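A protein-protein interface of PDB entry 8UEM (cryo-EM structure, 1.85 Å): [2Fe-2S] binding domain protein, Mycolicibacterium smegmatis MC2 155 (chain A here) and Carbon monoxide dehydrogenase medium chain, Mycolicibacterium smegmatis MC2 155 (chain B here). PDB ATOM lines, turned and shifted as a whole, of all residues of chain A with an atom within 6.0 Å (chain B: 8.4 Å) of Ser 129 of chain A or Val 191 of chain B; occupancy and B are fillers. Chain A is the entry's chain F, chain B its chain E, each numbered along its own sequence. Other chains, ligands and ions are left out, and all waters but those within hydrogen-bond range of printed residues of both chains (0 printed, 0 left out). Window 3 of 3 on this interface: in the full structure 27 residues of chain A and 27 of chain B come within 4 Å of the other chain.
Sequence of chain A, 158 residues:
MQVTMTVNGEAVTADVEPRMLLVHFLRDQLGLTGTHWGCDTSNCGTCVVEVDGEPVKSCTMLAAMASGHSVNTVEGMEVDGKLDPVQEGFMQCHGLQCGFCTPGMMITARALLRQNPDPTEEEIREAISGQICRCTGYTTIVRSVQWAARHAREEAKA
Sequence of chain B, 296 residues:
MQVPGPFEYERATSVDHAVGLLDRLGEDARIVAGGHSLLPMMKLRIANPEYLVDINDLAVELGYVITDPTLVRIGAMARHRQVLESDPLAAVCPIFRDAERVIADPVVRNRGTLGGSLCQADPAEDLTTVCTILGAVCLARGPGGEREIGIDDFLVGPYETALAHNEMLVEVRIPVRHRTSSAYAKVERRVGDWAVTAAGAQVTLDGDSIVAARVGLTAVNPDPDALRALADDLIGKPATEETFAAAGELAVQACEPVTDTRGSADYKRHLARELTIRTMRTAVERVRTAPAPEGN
Among the printed residues, pairs that only touch across the chains: Glu 126 of chain A with Pro 106 of chain B (3.1 Å), Gly 130 of chain A with Asp 105 of chain B (3.2 Å), Ser 129 of chain A with Pro 106 of chain B (3.3 Å), Gln 131 of chain A with Val 107 of chain B (3.5 Å), Ile 132 of chain A with Arg 190 of chain B (3.8 Å) and Ser 129 of chain A with Val 191 of chain B (3.8 Å).
Of the 9 printed residues of chain A, 5 touch a printed residue of chain B.
Hydrophobic or aromatic side chains of chain A that line the printed part of chain B: Ile 132.
Of the 17 printed residues of chain B, 5 touch a printed residue of chain A.
Hydrophobic or aromatic side chains of chain B that line the printed part of chain A: Pro 106, Val 107 and Val 191.
Among the printed residues, 6 pairs touch across the chains.
Among the printed residues, no Asp or Glu carboxylate lies within 4 Å of a Lys or Arg side-chain nitrogen of the other chain.
The backbone carbonyl oxygen (O) of Glu 126 of chain A sits at hydrogen-bond distance from the side-chain hydroxyl (OG) of Ser 129 of chain A, at 2.6 Å.
OD1 of Asp 105 of chain B sits close to N of Val 107 of chain B (3.2 Å).
Ser 129 of chain A touches two residues of chain B.
Of the printed residues of chain B, Ile 132 of chain A touches Arg 190 (3.8 Å).
Printed residues of chain A within 4 Å of Asp 105 of chain B: Gly 130.
Of the printed residues of chain A, Pro 106 of chain B touches Glu 126 and Ser 129.
Lys 186 of chain B touches none of the printed residues of chain A.
Of chain A, only Ser 129 comes within 4 Å of Val 191 of chain B.
The nearest residue of chain B that does not touch Ser 129 of chain A is Asp 105 of chain B (4.2 Å).
The nearest residue of chain A that does not touch Val 191 of chain B is Gly 130 of chain A (5.8 Å).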
ATOM      1  N   ILE A 124      16.469  25.658  -6.655  1.00  0.00           N
ATOM      2  CA  ILE A 124      16.399  27.117  -6.938  1.00  0.00           C
ATOM      3  C   ILE A 124      15.264  27.755  -6.145  1.00  0.00           C
ATOM      4  O   ILE A 124      15.513  28.763  -5.488  1.00  0.00           O
ATOM      5  CB  ILE A 124      16.297  27.416  -8.441  1.00  0.00           C
ATOM      6  CG1 ILE A 124      17.470  26.800  -9.207  1.00  0.00           C
ATOM      7  CG2 ILE A 124      16.138  28.904  -8.696  1.00  0.00           C
ATOM      8  CD1 ILE A 124      17.174  26.487 -10.648  1.00  0.00           C
ATOM      9  N   ARG A 125      14.096  27.128  -6.167  1.00  0.00           N
ATOM     10  CA  ARG A 125      12.937  27.675  -5.430  1.00  0.00           C
ATOM     11  C   ARG A 125      13.325  27.794  -3.961  1.00  0.00           C
ATOM     12  O   ARG A 125      13.149  28.853  -3.379  1.00  0.00           O
ATOM     13  CB  ARG A 125      11.735  26.763  -5.677  1.00  0.00           C
ATOM     14  CG  ARG A 125      11.215  26.916  -7.097  1.00  0.00           C
ATOM     15  CD  ARG A 125       9.912  26.223  -7.413  1.00  0.00           C
ATOM     16  NE  ARG A 125       9.500  26.462  -8.787  1.00  0.00           N
ATOM     17  CZ  ARG A 125       8.786  27.501  -9.205  1.00  0.00           C
ATOM     18  NH1 ARG A 125       8.398  28.439  -8.359  1.00  0.00           N
ATOM     19  NH2 ARG A 125       8.456  27.596 -10.478  1.00  0.00           N
ATOM     20  N   GLU A 126      13.862  26.707  -3.418  1.00  0.00           N
ATOM     21  CA  GLU A 126      14.224  26.725  -2.009  1.00  0.00           C
ATOM     22  C   GLU A 126      15.253  27.808  -1.730  1.00  0.00           C
ATOM     23  O   GLU A 126      15.127  28.557  -0.756  1.00  0.00           O
ATOM     24  CB  GLU A 126      14.753  25.352  -1.587  1.00  0.00           C
ATOM     25  CG  GLU A 126      13.684  24.277  -1.532  1.00  0.00           C
ATOM     26  CD  GLU A 126      14.250  22.900  -1.218  1.00  0.00           C
ATOM     27  OE1 GLU A 126      15.465  22.699  -1.411  1.00  0.00           O
ATOM     28  OE2 GLU A 126      13.478  22.020  -0.788  1.00  0.00           O
ATOM     29  N   ALA A 127      16.266  27.920  -2.592  1.00  0.00           N
ATOM     30  CA  ALA A 127      17.333  28.890  -2.370  1.00  0.00           C
ATOM     31  C   ALA A 127      16.809  30.314  -2.384  1.00  0.00           C
ATOM     32  O   ALA A 127      17.340  31.176  -1.684  1.00  0.00           O
ATOM     33  CB  ALA A 127      18.428  28.727  -3.420  1.00  0.00           C
ATOM     34  N   ILE A 128      15.776  30.584  -3.176  1.00  0.00           N
ATOM     35  CA  ILE A 128      15.199  31.916  -3.254  1.00  0.00           C
ATOM     36  C   ILE A 128      13.933  32.033  -2.418  1.00  0.00           C
ATOM     37  O   ILE A 128      13.249  33.055  -2.476  1.00  0.00           O
ATOM     38  CB  ILE A 128      14.936  32.311  -4.713  1.00  0.00           C
ATOM     39  CG1 ILE A 128      13.977  31.317  -5.377  1.00  0.00           C
ATOM     40  CG2 ILE A 128      16.249  32.404  -5.465  1.00  0.00           C
ATOM     41  CD1 ILE A 128      13.522  31.734  -6.747  1.00  0.00           C
ATOM     42  N   SER A 129      13.607  31.003  -1.641  1.00  0.00           N
ATOM     43  CA  SER A 129      12.346  30.968  -0.914  1.00  0.00           C
ATOM     44  C   SER A 129      12.261  32.043   0.155  1.00  0.00           C
ATOM     45  O   SER A 129      11.171  32.309   0.660  1.00  0.00           O
ATOM     46  CB  SER A 129      12.149  29.589  -0.289  1.00  0.00           C
ATOM     47  OG  SER A 129      13.120  29.341   0.707  1.00  0.00           O
ATOM     48  N   GLY A 130      13.380  32.648   0.520  1.00  0.00           N
ATOM     49  CA  GLY A 130      13.381  33.783   1.409  1.00  0.00           C
ATOM     50  C   GLY A 130      13.258  35.117   0.715  1.00  0.00           C
ATOM     51  O   GLY A 130      13.347  36.156   1.375  1.00  0.00           O
ATOM     52  N   GLN A 131      13.062  35.127  -0.599  1.00  0.00           N
ATOM     53  CA  GLN A 131      13.040  36.367  -1.362  1.00  0.00           C
ATOM     54  C   GLN A 131      11.761  36.453  -2.179  1.00  0.00           C
ATOM     55  O   GLN A 131      11.489  35.590  -3.018  1.00  0.00           O
ATOM     56  CB  GLN A 131      14.268  36.479  -2.261  1.00  0.00           C
ATOM     57  CG  GLN A 131      15.536  36.817  -1.491  1.00  0.00           C
ATOM     58  CD  GLN A 131      16.740  36.172  -2.088  1.00  0.00           C
ATOM     59  OE1 GLN A 131      17.333  35.274  -1.503  1.00  0.00           O
ATOM     60  NE2 GLN A 131      17.118  36.624  -3.270  1.00  0.00           N
ATOM     61  N   ILE A 132      11.004  37.504  -1.948  1.00  0.00           N
ATOM     62  CA  ILE A 132       9.703  37.678  -2.566  1.00  0.00           C
ATOM     63  C   ILE A 132       9.870  38.391  -3.897  1.00  0.00           C
ATOM     64  O   ILE A 132      10.512  39.441  -3.971  1.00  0.00           O
ATOM     65  CB  ILE A 132       8.772  38.472  -1.643  1.00  0.00           C
ATOM     66  CG1 ILE A 132       8.509  37.688  -0.359  1.00  0.00           C
ATOM     67  CG2 ILE A 132       7.495  38.855  -2.384  1.00  0.00           C
ATOM     68  CD1 ILE A 132       7.639  38.438   0.607  1.00  0.00           C
ATOM     69  N   ARG B 101      15.167  22.827   8.019  1.00  0.00           N
ATOM     70  CA  ARG B 101      14.617  22.924   6.674  1.00  0.00           C
ATOM     71  C   ARG B 101      13.356  23.772   6.645  1.00  0.00           C
ATOM     72  O   ARG B 101      13.048  24.390   5.622  1.00  0.00           O
ATOM     73  CB  ARG B 101      14.335  21.528   6.123  1.00  0.00           C
ATOM     74  CG  ARG B 101      15.591  20.763   5.788  1.00  0.00           C
ATOM     75  CD  ARG B 101      15.352  19.740   4.705  1.00  0.00           C
ATOM     76  NE  ARG B 101      15.153  18.404   5.248  1.00  0.00           N
ATOM     77  CZ  ARG B 101      15.934  17.367   4.984  1.00  0.00           C
ATOM     78  NH1 ARG B 101      16.992  17.482   4.198  1.00  0.00           N
ATOM     79  NH2 ARG B 101      15.648  16.185   5.523  1.00  0.00           N
ATOM     80  N   VAL B 102      12.673  23.869   7.776  1.00  0.00           N
ATOM     81  CA  VAL B 102      11.362  24.576   7.807  1.00  0.00           C
ATOM     82  C   VAL B 102      11.464  25.816   8.681  1.00  0.00           C
ATOM     83  O   VAL B 102      10.428  26.399   8.997  1.00  0.00           O
ATOM     84  CB  VAL B 102      10.232  23.596   8.204  1.00  0.00           C
ATOM     85  CG1 VAL B 102      10.014  22.521   7.154  1.00  0.00           C
ATOM     86  CG2 VAL B 102      10.440  22.985   9.578  1.00  0.00           C
ATOM     87  N   ILE B 103      12.700  26.184   9.021  1.00  0.00           N
ATOM     88  CA  ILE B 103      12.920  27.411   9.831  1.00  0.00           C
ATOM     89  C   ILE B 103      13.257  28.564   8.908  1.00  0.00           C
ATOM     90  O   ILE B 103      14.181  28.389   8.115  1.00  0.00           O
ATOM     91  CB  ILE B 103      13.989  27.269  10.936  1.00  0.00           C
ATOM     92  CG1 ILE B 103      13.503  26.389  12.087  1.00  0.00           C
ATOM     93  CG2 ILE B 103      14.439  28.630  11.437  1.00  0.00           C
ATOM     94  CD1 ILE B 103      14.604  25.999  13.024  1.00  0.00           C
ATOM     95  N   ALA B 104      12.501  29.642   8.992  1.00  0.00           N
ATOM     96  CA  ALA B 104      12.819  30.884   8.294  1.00  0.00           C
ATOM     97  C   ALA B 104      13.084  30.541   6.828  1.00  0.00           C
ATOM     98  O   ALA B 104      12.324  29.766   6.234  1.00  0.00           O
ATOM     99  CB  ALA B 104      13.962  31.583   9.020  1.00  0.00           C
ATOM    100  N   ASP B 105      14.121  31.072   6.219  1.00  0.00           N
ATOM    101  CA  ASP B 105      14.482  30.788   4.842  1.00  0.00           C
ATOM    102  C   ASP B 105      15.994  30.618   4.796  1.00  0.00           C
ATOM    103  O   ASP B 105      16.669  30.884   5.796  1.00  0.00           O
ATOM    104  CB  ASP B 105      14.014  31.917   3.924  1.00  0.00           C
ATOM    105  CG  ASP B 105      14.382  33.285   4.456  1.00  0.00           C
ATOM    106  OD1 ASP B 105      15.587  33.580   4.537  1.00  0.00           O
ATOM    107  OD2 ASP B 105      13.472  34.063   4.803  1.00  0.00           O
ATOM    108  N   PRO B 106      16.562  30.178   3.673  1.00  0.00           N
ATOM    109  CA  PRO B 106      18.018  29.945   3.646  1.00  0.00           C
ATOM    110  C   PRO B 106      18.836  31.168   4.033  1.00  0.00           C
ATOM    111  O   PRO B 106      19.845  31.037   4.741  1.00  0.00           O
ATOM    112  CB  PRO B 106      18.273  29.520   2.194  1.00  0.00           C
ATOM    113  CG  PRO B 106      16.962  28.982   1.723  1.00  0.00           C
ATOM    114  CD  PRO B 106      15.916  29.813   2.402  1.00  0.00           C
ATOM    115  N   VAL B 107      18.423  32.360   3.609  1.00  0.00           N
ATOM    116  CA  VAL B 107      19.199  33.551   3.935  1.00  0.00           C
ATOM    117  C   VAL B 107      19.230  33.761   5.443  1.00  0.00           C
ATOM    118  O   VAL B 107      20.286  34.012   6.028  1.00  0.00           O
ATOM    119  CB  VAL B 107      18.646  34.783   3.196  1.00  0.00           C
ATOM    120  CG1 VAL B 107      19.508  35.991   3.486  1.00  0.00           C
ATOM    121  CG2 VAL B 107      18.605  34.525   1.702  1.00  0.00           C
ATOM    122  N   ARG B 109      18.760  31.497   7.707  1.00  0.00           N
ATOM    123  CA  ARG B 109      19.552  30.373   8.248  1.00  0.00           C
ATOM    124  C   ARG B 109      21.054  30.660   8.162  1.00  0.00           C
ATOM    125  O   ARG B 109      21.799  30.081   8.945  1.00  0.00           O
ATOM    126  CB  ARG B 109      19.137  29.062   7.598  1.00  0.00           C
ATOM    127  CG  ARG B 109      17.726  28.662   7.998  1.00  0.00           C
ATOM    128  CD  ARG B 109      17.456  27.202   7.740  1.00  0.00           C
ATOM    129  NE  ARG B 109      17.577  26.871   6.337  1.00  0.00           N
ATOM    130  CZ  ARG B 109      16.583  26.888   5.462  1.00  0.00           C
ATOM    131  NH1 ARG B 109      15.366  27.242   5.835  1.00  0.00           N
ATOM    132  NH2 ARG B 109      16.817  26.557   4.209  1.00  0.00           N
ATOM    133  N   LYS B 186       6.258  20.645  10.869  1.00  0.00           N
ATOM    134  CA  LYS B 186       5.738  21.964  11.136  1.00  0.00           C
ATOM    135  C   LYS B 186       4.670  22.293  10.116  1.00  0.00           C
ATOM    136  O   LYS B 186       4.783  21.861   8.982  1.00  0.00           O
ATOM    137  CB  LYS B 186       6.869  22.968  11.008  1.00  0.00           C
ATOM    138  CG  LYS B 186       6.460  24.418  11.052  1.00  0.00           C
ATOM    139  CD  LYS B 186       7.684  25.237  11.189  1.00  0.00           C
ATOM    140  CE  LYS B 186       7.497  26.593  10.578  1.00  0.00           C
ATOM    141  NZ  LYS B 186       8.530  27.489  11.115  1.00  0.00           N
ATOM    142  N   VAL B 187       3.622  22.918  10.574  1.00  0.00           N
ATOM    143  CA  VAL B 187       2.625  23.470   9.677  1.00  0.00           C
ATOM    144  C   VAL B 187       2.703  24.979   9.792  1.00  0.00           C
ATOM    145  O   VAL B 187       2.511  25.548  10.880  1.00  0.00           O
ATOM    146  CB  VAL B 187       1.210  22.964   9.979  1.00  0.00           C
ATOM    147  CG1 VAL B 187       0.197  23.852   9.280  1.00  0.00           C
ATOM    148  CG2 VAL B 187       1.061  21.532   9.514  1.00  0.00           C
ATOM    149  N   GLU B 188       2.978  25.603   8.656  1.00  0.00           N
ATOM    150  CA  GLU B 188       3.057  27.037   8.478  1.00  0.00           C
ATOM    151  C   GLU B 188       2.158  27.419   7.312  1.00  0.00           C
ATOM    152  O   GLU B 188       1.949  26.629   6.390  1.00  0.00           O
ATOM    153  CB  GLU B 188       4.502  27.465   8.202  1.00  0.00           C
ATOM    154  CG  GLU B 188       5.046  26.929   6.886  1.00  0.00           C
ATOM    155  CD  GLU B 188       6.279  26.069   7.059  1.00  0.00           C
ATOM    156  OE1 GLU B 188       6.239  25.112   7.857  1.00  0.00           O
ATOM    157  OE2 GLU B 188       7.290  26.349   6.384  1.00  0.00           O
ATOM    158  N   ARG B 189       1.607  28.630   7.361  1.00  0.00           N
ATOM    159  CA  ARG B 189       0.818  29.096   6.228  1.00  0.00           C
ATOM    160  C   ARG B 189       1.680  29.238   4.984  1.00  0.00           C
ATOM    161  O   ARG B 189       1.211  28.995   3.868  1.00  0.00           O
ATOM    162  CB  ARG B 189       0.142  30.419   6.568  1.00  0.00           C
ATOM    163  CG  ARG B 189      -0.927  30.310   7.633  1.00  0.00           C
ATOM    164  CD  ARG B 189      -1.107  31.613   8.367  1.00  0.00           C
ATOM    165  NE  ARG B 189       0.155  32.121   8.887  1.00  0.00           N
ATOM    166  CZ  ARG B 189       0.354  33.376   9.260  1.00  0.00           C
ATOM    167  NH1 ARG B 189      -0.606  34.279   9.178  1.00  0.00           N
ATOM    168  NH2 ARG B 189       1.542  33.730   9.735  1.00  0.00           N
ATOM    169  N   ARG B 190       2.944  29.608   5.161  1.00  0.00           N
ATOM    170  CA  ARG B 190       3.846  29.875   4.055  1.00  0.00           C
ATOM    171  C   ARG B 190       5.252  29.456   4.450  1.00  0.00           C
ATOM    172  O   ARG B 190       5.606  29.430   5.630  1.00  0.00           O
ATOM    173  CB  ARG B 190       3.832  31.355   3.662  1.00  0.00           C
ATOM    174  CG  ARG B 190       4.575  31.645   2.384  1.00  0.00           C
ATOM    175  CD  ARG B 190       4.729  33.131   2.173  1.00  0.00           C
ATOM    176  NE  ARG B 190       5.396  33.792   3.288  1.00  0.00           N
ATOM    177  CZ  ARG B 190       6.380  34.670   3.158  1.00  0.00           C
ATOM    178  NH1 ARG B 190       6.835  35.030   1.972  1.00  0.00           N
ATOM    179  NH2 ARG B 190       6.920  35.205   4.249  1.00  0.00           N
ATOM    180  N   VAL B 191       6.058  29.139   3.438  1.00  0.00           N
ATOM    181  CA  VAL B 191       7.459  28.831   3.680  1.00  0.00           C
ATOM    182  C   VAL B 191       8.124  30.032   4.330  1.00  0.00           C
ATOM    183  O   VAL B 191       7.970  31.173   3.878  1.00  0.00           O
ATOM    184  CB  VAL B 191       8.154  28.438   2.368  1.00  0.00           C
ATOM    185  CG1 VAL B 191       9.647  28.678   2.462  1.00  0.00           C
ATOM    186  CG2 VAL B 191       7.858  26.992   2.030  1.00  0.00           C
ATOM    187  N   GLY B 192       8.851  29.785   5.414  1.00  0.00           N
ATOM    188  CA  GLY B 192       9.449  30.841   6.192  1.00  0.00           C
ATOM    189  C   GLY B 192       8.554  31.401   7.275  1.00  0.00           C
ATOM    190  O   GLY B 192       9.048  32.078   8.182  1.00  0.00           O
ATOM    191  N   ASP B 193       7.255  31.133   7.206  1.00  0.00           N
ATOM    192  CA  ASP B 193       6.344  31.563   8.249  1.00  0.00           C
ATOM    193  C   ASP B 193       6.582  30.746   9.512  1.00  0.00           C
ATOM    194  O   ASP B 193       6.994  29.584   9.464  1.00  0.00           O
ATOM    195  CB  ASP B 193       4.896  31.419   7.778  1.00  0.00           C
ATOM    196  CG  ASP B 193       3.895  31.852   8.828  1.00  0.00           C
ATOM    197  OD1 ASP B 193       4.162  32.845   9.528  1.00  0.00           O
ATOM    198  OD2 ASP B 193       2.843  31.193   8.951  1.00  0.00           O
ATOM    199  N   TRP B 194       6.350  31.378  10.655  1.00  0.00           N
ATOM    200  CA  TRP B 194       6.457  30.668  11.914  1.00  0.00           C
ATOM    201  C   TRP B 194       5.404  29.570  11.978  1.00  0.00           C
ATOM    202  O   TRP B 194       4.378  29.619  11.300  1.00  0.00           O
ATOM    203  CB  TRP B 194       6.293  31.631  13.082  1.00  0.00           C
ATOM    204  CG  TRP B 194       7.567  32.298  13.461  1.00  0.00           C
ATOM    205  CD1 TRP B 194       8.388  31.970  14.491  1.00  0.00           C
ATOM    206  CD2 TRP B 194       8.163  33.421  12.812  1.00  0.00           C
ATOM    207  NE1 TRP B 194       9.464  32.818  14.526  1.00  0.00           N
ATOM    208  CE2 TRP B 194       9.349  33.719  13.504  1.00  0.00           C
ATOM    209  CE3 TRP B 194       7.811  34.201  11.710  1.00  0.00           C
ATOM    210  CZ2 TRP B 194      10.182  34.766  13.135  1.00  0.00           C
ATOM    211  CZ3 TRP B 194       8.642  35.242  11.345  1.00  0.00           C
ATOM    212  CH2 TRP B 194       9.817  35.512  12.055  1.00  0.00           C
